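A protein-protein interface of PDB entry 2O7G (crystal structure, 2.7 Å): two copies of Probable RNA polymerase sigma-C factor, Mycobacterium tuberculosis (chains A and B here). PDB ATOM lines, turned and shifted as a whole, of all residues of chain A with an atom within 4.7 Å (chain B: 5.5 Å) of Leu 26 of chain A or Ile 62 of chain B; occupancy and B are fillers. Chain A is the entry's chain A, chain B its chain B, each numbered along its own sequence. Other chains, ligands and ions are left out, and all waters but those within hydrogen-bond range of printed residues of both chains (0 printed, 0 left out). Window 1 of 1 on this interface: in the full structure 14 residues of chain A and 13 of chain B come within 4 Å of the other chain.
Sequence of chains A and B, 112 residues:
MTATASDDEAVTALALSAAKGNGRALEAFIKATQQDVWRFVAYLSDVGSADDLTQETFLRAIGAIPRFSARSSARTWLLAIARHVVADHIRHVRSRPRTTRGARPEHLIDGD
Leu 26 of chain A touches Ile 62 of chain B, and with the chains exchanged Ile 62 of chain A touches Leu 26 of chain B. Ile 30 of chain A touches Ile 62 of chain B, and with the chains exchanged Ile 62 of chain A touches Ile 30 of chain B. Ile 62 of chain A touches its own counterpart, Ile 62 of chain B. Positions printed for both chains: 26, 30, 62 and 65. Of the 14 pairs that touch across the chains among the printed residues, 5 have their exchanged pair printed and touching as well.
Of the printed residues of chain B, Gly 23 of chain A touches Ile 62 (3.4 Å), Gly 63 (3.6 Å) and Pro 66 (3.7 Å). Ala 25 of chain A touches none of the printed residues of chain B. Leu 26 of chain A touches just one residue of chain B: Ile 62 (3.3 Å). Phe 29 of chain A touches none of the printed residues of chain B. Of the printed residues of chain B, Ile 30 of chain A touches Leu 59 (3.8 Å) and Ile 62 (3.9 Å). Of the printed residues of chain B, Ile 62 of chain A touches Leu 26 (3.5 Å), Ile 30 (3.9 Å) and Ile 62 (3.9 Å). Ile 62 of chain B touches just these residues of chain A: Gly 23 (3.4 Å), Leu 26 (3.3 Å), Glu 27 (3.9 Å), Ile 30 (3.9 Å) and Ile 62 (3.9 Å). The nearest residue of chain B that does not touch Leu 26 of chain A is Leu 26 of chain B (4.4 Å).
O of Leu 59 of chain B lies close to OE1 of Glu 27 of chain A (3.1 Å).
Among the printed residues, merely in contact across the chains: Gly 23 of chain A with Ile 62 of chain B (3.4 Å), Gly 23 of chain A with Gly 63 of chain B (3.6 Å), Gly 23 of chain A with Pro 66 of chain B (3.7 Å), Arg 24 of chain A with Gly 63 of chain B (3.8 Å), Leu 26 of chain A with Ile 62 of chain B (3.3 Å), Glu 27 of chain A with Arg 60 of chain B (3.8 Å), Glu 27 of chain A with Ile 62 of chain B (3.9 Å), Glu 27 of chain A with Gly 63 of chain B (3.5 Å), Ile 30 of chain A with Leu 59 of chain B (3.8 Å), Ile 30 of chain A with Ile 62 of chain B (3.9 Å), Ile 62 of chain A with Leu 26 of chain B (3.5 Å), Ile 62 of chain A with Ile 30 of chain B (3.9 Å) and Ile 62 of chain A with Ile 62 of chain B (3.9 Å).
Of the 12 printed residues of chain A, 6 touch a printed residue of chain B. Printed residues of chain A that touch a printed residue of chain B: Gly 23, Arg 24, Leu 26, Glu 27, Ile 30 and Ile 62. Of the 12 printed residues of chain B, 7 touch a printed residue of chain A. Printed residues of chain B that touch a printed residue of chain A: Leu 26, Ile 30, Leu 59, Arg 60, Ile 62, Gly 63 and Pro 66. Among the printed residues, no Asp or Glu carboxylate lies within 4 Å of a Lys or Arg side-chain nitrogen of the other chain.
The side-chain amide oxygen (OD1) of Asn 22 of chain A sits at hydrogen-bond distance from the backbone NH (N) of Arg 24 of chain A, at 2.9 Å.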
ATOM      1  N   ALA A  18      -1.094  18.076  10.674  1.00  0.00           N
ATOM      2  CA  ALA A  18      -1.632  16.916   9.978  1.00  0.00           C
ATOM      3  C   ALA A  18      -0.514  16.021   9.445  1.00  0.00           C
ATOM      4  O   ALA A  18      -0.579  14.833   9.629  1.00  0.00           O
ATOM      5  CB  ALA A  18      -2.548  17.326   8.859  1.00  0.00           C
ATOM      6  N   ASN A  22      -1.670  14.291  13.172  1.00  0.00           N
ATOM      7  CA  ASN A  22      -2.867  14.821  13.823  1.00  0.00           C
ATOM      8  C   ASN A  22      -4.121  14.803  12.898  1.00  0.00           C
ATOM      9  O   ASN A  22      -4.251  15.603  11.967  1.00  0.00           O
ATOM     10  CB  ASN A  22      -2.618  16.237  14.371  1.00  0.00           C
ATOM     11  CG  ASN A  22      -3.738  16.695  15.289  1.00  0.00           C
ATOM     12  OD1 ASN A  22      -4.858  16.897  14.932  1.00  0.00           O
ATOM     13  ND2 ASN A  22      -3.436  16.798  16.470  1.00  0.00           N
ATOM     14  N   GLY A  23      -5.058  13.906  13.166  1.00  0.00           N
ATOM     15  CA  GLY A  23      -6.275  13.819  12.391  1.00  0.00           C
ATOM     16  C   GLY A  23      -7.180  15.047  12.474  1.00  0.00           C
ATOM     17  O   GLY A  23      -7.827  15.401  11.453  1.00  0.00           O
ATOM     18  N   ARG A  24      -7.238  15.717  13.659  1.00  0.00           N
ATOM     19  CA  ARG A  24      -8.121  16.894  13.767  1.00  0.00           C
ATOM     20  C   ARG A  24      -7.585  18.104  12.971  1.00  0.00           C
ATOM     21  O   ARG A  24      -8.346  18.963  12.474  1.00  0.00           O
ATOM     22  CB  ARG A  24      -8.481  17.301  15.193  1.00  0.00           C
ATOM     23  CG  ARG A  24      -8.799  16.225  16.183  1.00  0.00           C
ATOM     24  CD  ARG A  24      -9.968  16.590  17.167  1.00  0.00           C
ATOM     25  NE  ARG A  24     -10.791  15.372  17.003  1.00  0.00           N
ATOM     26  CZ  ARG A  24     -11.067  14.379  17.894  1.00  0.00           C
ATOM     27  NH1 ARG A  24     -11.695  13.291  17.516  1.00  0.00           N
ATOM     28  NH2 ARG A  24     -10.780  14.428  19.170  1.00  0.00           N
ATOM     29  N   ALA A  25      -6.265  18.150  12.860  1.00  0.00           N
ATOM     30  CA  ALA A  25      -5.589  19.122  12.057  1.00  0.00           C
ATOM     31  C   ALA A  25      -5.945  18.817  10.599  1.00  0.00           C
ATOM     32  O   ALA A  25      -6.388  19.734   9.881  1.00  0.00           O
ATOM     33  CB  ALA A  25      -4.069  19.085  12.313  1.00  0.00           C
ATOM     34  N   LEU A  26      -5.820  17.548  10.173  1.00  0.00           N
ATOM     35  CA  LEU A  26      -6.138  17.185   8.797  1.00  0.00           C
ATOM     36  C   LEU A  26      -7.584  17.529   8.480  1.00  0.00           C
ATOM     37  O   LEU A  26      -7.889  18.117   7.461  1.00  0.00           O
ATOM     38  CB  LEU A  26      -5.994  15.714   8.616  1.00  0.00           C
ATOM     39  CG  LEU A  26      -5.355  15.138   7.364  1.00  0.00           C
ATOM     40  CD1 LEU A  26      -6.126  14.142   6.898  1.00  0.00           C
ATOM     41  CD2 LEU A  26      -5.254  15.979   6.223  1.00  0.00           C
ATOM     42  N   GLU A  27      -8.487  17.175   9.367  1.00  0.00           N
ATOM     43  CA  GLU A  27      -9.851  17.452   9.096  1.00  0.00           C
ATOM     44  C   GLU A  27     -10.081  18.954   8.889  1.00  0.00           C
ATOM     45  O   GLU A  27     -10.722  19.369   7.903  1.00  0.00           O
ATOM     46  CB  GLU A  27     -10.704  16.916  10.238  1.00  0.00           C
ATOM     47  CG  GLU A  27     -12.160  17.240  10.113  1.00  0.00           C
ATOM     48  CD  GLU A  27     -12.963  16.728  11.317  1.00  0.00           C
ATOM     49  OE1 GLU A  27     -12.441  16.112  12.254  1.00  0.00           O
ATOM     50  OE2 GLU A  27     -14.158  16.899  11.354  1.00  0.00           O
ATOM     51  N   ALA A  28      -9.592  19.750   9.848  1.00  0.00           N
ATOM     52  CA  ALA A  28      -9.743  21.208   9.863  1.00  0.00           C
ATOM     53  C   ALA A  28      -9.114  21.807   8.591  1.00  0.00           C
ATOM     54  O   ALA A  28      -9.723  22.633   7.949  1.00  0.00           O
ATOM     55  CB  ALA A  28      -9.102  21.770  11.121  1.00  0.00           C
ATOM     56  N   PHE A  29      -7.935  21.336   8.205  1.00  0.00           N
ATOM     57  CA  PHE A  29      -7.298  21.765   6.983  1.00  0.00           C
ATOM     58  C   PHE A  29      -8.189  21.572   5.761  1.00  0.00           C
ATOM     59  O   PHE A  29      -8.260  22.459   4.871  1.00  0.00           O
ATOM     60  CB  PHE A  29      -6.026  20.964   6.819  1.00  0.00           C
ATOM     61  CG  PHE A  29      -5.332  21.159   5.507  1.00  0.00           C
ATOM     62  CD1 PHE A  29      -4.499  22.257   5.301  1.00  0.00           C
ATOM     63  CD2 PHE A  29      -5.446  20.186   4.494  1.00  0.00           C
ATOM     64  CE1 PHE A  29      -3.818  22.409   4.094  1.00  0.00           C
ATOM     65  CE2 PHE A  29      -4.783  20.331   3.257  1.00  0.00           C
ATOM     66  CZ  PHE A  29      -3.963  21.446   3.058  1.00  0.00           C
ATOM     67  N   ILE A  30      -8.856  20.418   5.687  1.00  0.00           N
ATOM     68  CA  ILE A  30      -9.751  20.135   4.558  1.00  0.00           C
ATOM     69  C   ILE A  30     -10.955  21.046   4.555  1.00  0.00           C
ATOM     70  O   ILE A  30     -11.309  21.611   3.523  1.00  0.00           O
ATOM     71  CB  ILE A  30     -10.204  18.700   4.528  1.00  0.00           C
ATOM     72  CG1 ILE A  30      -9.034  17.788   4.123  1.00  0.00           C
ATOM     73  CG2 ILE A  30     -11.392  18.535   3.571  1.00  0.00           C
ATOM     74  CD1 ILE A  30      -9.279  16.341   4.427  1.00  0.00           C
ATOM     75  N   ILE A  62      -4.471  13.812   1.132  1.00  0.00           N
ATOM     76  CA  ILE A  62      -4.395  12.965   2.331  1.00  0.00           C
ATOM     77  C   ILE A  62      -3.174  12.033   2.226  1.00  0.00           C
ATOM     78  O   ILE A  62      -2.362  11.912   3.152  1.00  0.00           O
ATOM     79  CB  ILE A  62      -5.698  12.200   2.566  1.00  0.00           C
ATOM     80  CG1 ILE A  62      -6.768  13.127   3.109  1.00  0.00           C
ATOM     81  CG2 ILE A  62      -5.496  11.080   3.556  1.00  0.00           C
ATOM     82  CD1 ILE A  62      -8.196  12.650   2.718  1.00  0.00           C
ATOM     83  N   ILE A  65       0.281  14.246   2.506  1.00  0.00           N
ATOM     84  CA  ILE A  65       0.492  15.226   3.509  1.00  0.00           C
ATOM     85  C   ILE A  65       1.564  14.914   4.490  1.00  0.00           C
ATOM     86  O   ILE A  65       2.111  15.789   5.087  1.00  0.00           O
ATOM     87  CB  ILE A  65      -0.784  15.769   4.116  1.00  0.00           C
ATOM     88  CG1 ILE A  65      -0.557  17.149   4.669  1.00  0.00           C
ATOM     89  CG2 ILE A  65      -1.305  14.916   5.146  1.00  0.00           C
ATOM     90  CD1 ILE A  65      -1.777  17.826   5.007  1.00  0.00           C
ATOM     91  N   LEU B  26      -4.686   6.013   4.789  1.00  0.00           N
ATOM     92  CA  LEU B  26      -5.936   6.724   4.978  1.00  0.00           C
ATOM     93  C   LEU B  26      -6.659   6.928   3.648  1.00  0.00           C
ATOM     94  O   LEU B  26      -7.880   6.707   3.533  1.00  0.00           O
ATOM     95  CB  LEU B  26      -5.634   8.049   5.625  1.00  0.00           C
ATOM     96  CG  LEU B  26      -6.765   8.966   6.062  1.00  0.00           C
ATOM     97  CD1 LEU B  26      -7.877   8.255   6.602  1.00  0.00           C
ATOM     98  CD2 LEU B  26      -6.358   9.748   7.137  1.00  0.00           C
ATOM     99  N   ILE B  30     -10.404   5.426   2.637  1.00  0.00           N
ATOM    100  CA  ILE B  30     -11.590   6.205   2.269  1.00  0.00           C
ATOM    101  C   ILE B  30     -12.128   5.719   0.933  1.00  0.00           C
ATOM    102  O   ILE B  30     -13.334   5.494   0.800  1.00  0.00           O
ATOM    103  CB  ILE B  30     -11.295   7.673   2.192  1.00  0.00           C
ATOM    104  CG1 ILE B  30     -11.033   8.231   3.585  1.00  0.00           C
ATOM    105  CG2 ILE B  30     -12.433   8.435   1.468  1.00  0.00           C
ATOM    106  CD1 ILE B  30     -10.475   9.625   3.521  1.00  0.00           C
ATOM    107  N   THR B  57     -19.160  12.315   7.383  1.00  0.00           N
ATOM    108  CA  THR B  57     -18.700  11.088   7.965  1.00  0.00           C
ATOM    109  C   THR B  57     -17.210  10.862   7.852  1.00  0.00           C
ATOM    110  O   THR B  57     -16.587  10.450   8.775  1.00  0.00           O
ATOM    111  CB  THR B  57     -19.427   9.938   7.345  1.00  0.00           C
ATOM    112  OG1 THR B  57     -20.812  10.158   7.445  1.00  0.00           O
ATOM    113  CG2 THR B  57     -19.094   8.670   8.006  1.00  0.00           C
ATOM    114  N   PHE B  58     -16.657  11.114   6.695  1.00  0.00           N
ATOM    115  CA  PHE B  58     -15.241  10.989   6.481  1.00  0.00           C
ATOM    116  C   PHE B  58     -14.401  12.038   7.190  1.00  0.00           C
ATOM    117  O   PHE B  58     -13.316  11.718   7.685  1.00  0.00           O
ATOM    118  CB  PHE B  58     -14.940  10.891   5.025  1.00  0.00           C
ATOM    119  CG  PHE B  58     -15.191   9.505   4.495  1.00  0.00           C
ATOM    120  CD1 PHE B  58     -16.166   9.257   3.507  1.00  0.00           C
ATOM    121  CD2 PHE B  58     -14.486   8.399   5.030  1.00  0.00           C
ATOM    122  CE1 PHE B  58     -16.410   7.954   3.046  1.00  0.00           C
ATOM    123  CE2 PHE B  58     -14.753   7.117   4.570  1.00  0.00           C
ATOM    124  CZ  PHE B  58     -15.710   6.889   3.567  1.00  0.00           C
ATOM    125  N   LEU B  59     -14.895  13.286   7.269  1.00  0.00           N
ATOM    126  CA  LEU B  59     -14.196  14.320   8.028  1.00  0.00           C
ATOM    127  C   LEU B  59     -14.086  13.931   9.504  1.00  0.00           C
ATOM    128  O   LEU B  59     -12.968  13.962  10.085  1.00  0.00           O
ATOM    129  CB  LEU B  59     -14.883  15.634   7.885  1.00  0.00           C
ATOM    130  CG  LEU B  59     -14.774  16.189   6.457  1.00  0.00           C
ATOM    131  CD1 LEU B  59     -15.581  17.314   6.318  1.00  0.00           C
ATOM    132  CD2 LEU B  59     -13.519  16.712   6.097  1.00  0.00           C
ATOM    133  N   ARG B  60     -15.186  13.451  10.097  1.00  0.00           N
ATOM    134  CA  ARG B  60     -15.070  12.936  11.459  1.00  0.00           C
ATOM    135  C   ARG B  60     -14.190  11.735  11.490  1.00  0.00           C
ATOM    136  O   ARG B  60     -13.390  11.597  12.407  1.00  0.00           O
ATOM    137  CB  ARG B  60     -16.404  12.569  12.063  1.00  0.00           C
ATOM    138  CG  ARG B  60     -17.432  13.566  11.844  1.00  0.00           C
ATOM    139  CD  ARG B  60     -18.242  13.733  13.040  1.00  0.00           C
ATOM    140  NE  ARG B  60     -19.408  14.514  12.678  1.00  0.00           N
ATOM    141  CZ  ARG B  60     -20.642  14.431  13.174  1.00  0.00           C
ATOM    142  NH1 ARG B  60     -20.995  13.542  14.121  1.00  0.00           N
ATOM    143  NH2 ARG B  60     -21.542  15.272  12.674  1.00  0.00           N
ATOM    144  N   ALA B  61     -14.320  10.844  10.500  1.00  0.00           N
ATOM    145  CA  ALA B  61     -13.446   9.657  10.472  1.00  0.00           C
ATOM    146  C   ALA B  61     -11.992  10.140  10.495  1.00  0.00           C
ATOM    147  O   ALA B  61     -11.187   9.678  11.283  1.00  0.00           O
ATOM    148  CB  ALA B  61     -13.732   8.758   9.240  1.00  0.00           C
ATOM    149  N   ILE B  62     -11.668  11.081   9.616  1.00  0.00           N
ATOM    150  CA  ILE B  62     -10.312  11.573   9.522  1.00  0.00           C
ATOM    151  C   ILE B  62      -9.831  12.070  10.885  1.00  0.00           C
ATOM    152  O   ILE B  62      -8.705  11.777  11.256  1.00  0.00           O
ATOM    153  CB  ILE B  62     -10.139  12.652   8.434  1.00  0.00           C
ATOM    154  CG1 ILE B  62     -10.082  12.000   7.053  1.00  0.00           C
ATOM    155  CG2 ILE B  62      -8.846  13.334   8.615  1.00  0.00           C
ATOM    156  CD1 ILE B  62     -10.410  12.940   5.907  1.00  0.00           C
ATOM    157  N   GLY B  63     -10.708  12.759  11.625  1.00  0.00           N
ATOM    158  CA  GLY B  63     -10.407  13.287  12.930  1.00  0.00           C
ATOM    159  C   GLY B  63     -10.173  12.208  13.952  1.00  0.00           C
ATOM    160  O   GLY B  63      -9.262  12.354  14.772  1.00  0.00           O
ATOM    161  N   ALA B  64     -10.969  11.123  13.924  1.00  0.00           N
ATOM    162  CA  ALA B  64     -10.965  10.081  15.001  1.00  0.00           C
ATOM    163  C   ALA B  64     -10.005   8.919  14.767  1.00  0.00           C
ATOM    164  O   ALA B  64      -9.634   8.169  15.685  1.00  0.00           O
ATOM    165  CB  ALA B  64     -12.318   9.562  15.160  1.00  0.00           C
ATOM    166  N   ILE B  65      -9.604   8.755  13.513  1.00  0.00           N
ATOM    167  CA  ILE B  65      -8.813   7.611  13.154  1.00  0.00           C
ATOM    168  C   ILE B  65      -7.538   7.483  13.981  1.00  0.00           C
ATOM    169  O   ILE B  65      -7.199   6.364  14.331  1.00  0.00           O
ATOM    170  CB  ILE B  65      -8.580   7.434  11.616  1.00  0.00           C
ATOM    171  CG1 ILE B  65      -8.258   5.955  11.302  1.00  0.00           C
ATOM    172  CG2 ILE B  65      -7.489   8.304  11.112  1.00  0.00           C
ATOM    173  CD1 ILE B  65      -9.020   5.435  10.103  1.00  0.00           C
ATOM    174  N   PRO B  66      -6.820   8.595  14.309  1.00  0.00           N
ATOM    175  CA  PRO B  66      -5.673   8.330  15.197  1.00  0.00           C
ATOM    176  C   PRO B  66      -5.975   7.513  16.447  1.00  0.00           C
ATOM    177  O   PRO B  66      -5.094   7.083  17.020  1.00  0.00           O
ATOM    178  CB  PRO B  66      -5.223   9.714  15.620  1.00  0.00           C
ATOM    179  CG  PRO B  66      -5.657  10.592  14.582  1.00  0.00           C
ATOM    180  CD  PRO B  66      -6.880  10.021  13.947  1.00  0.00           C
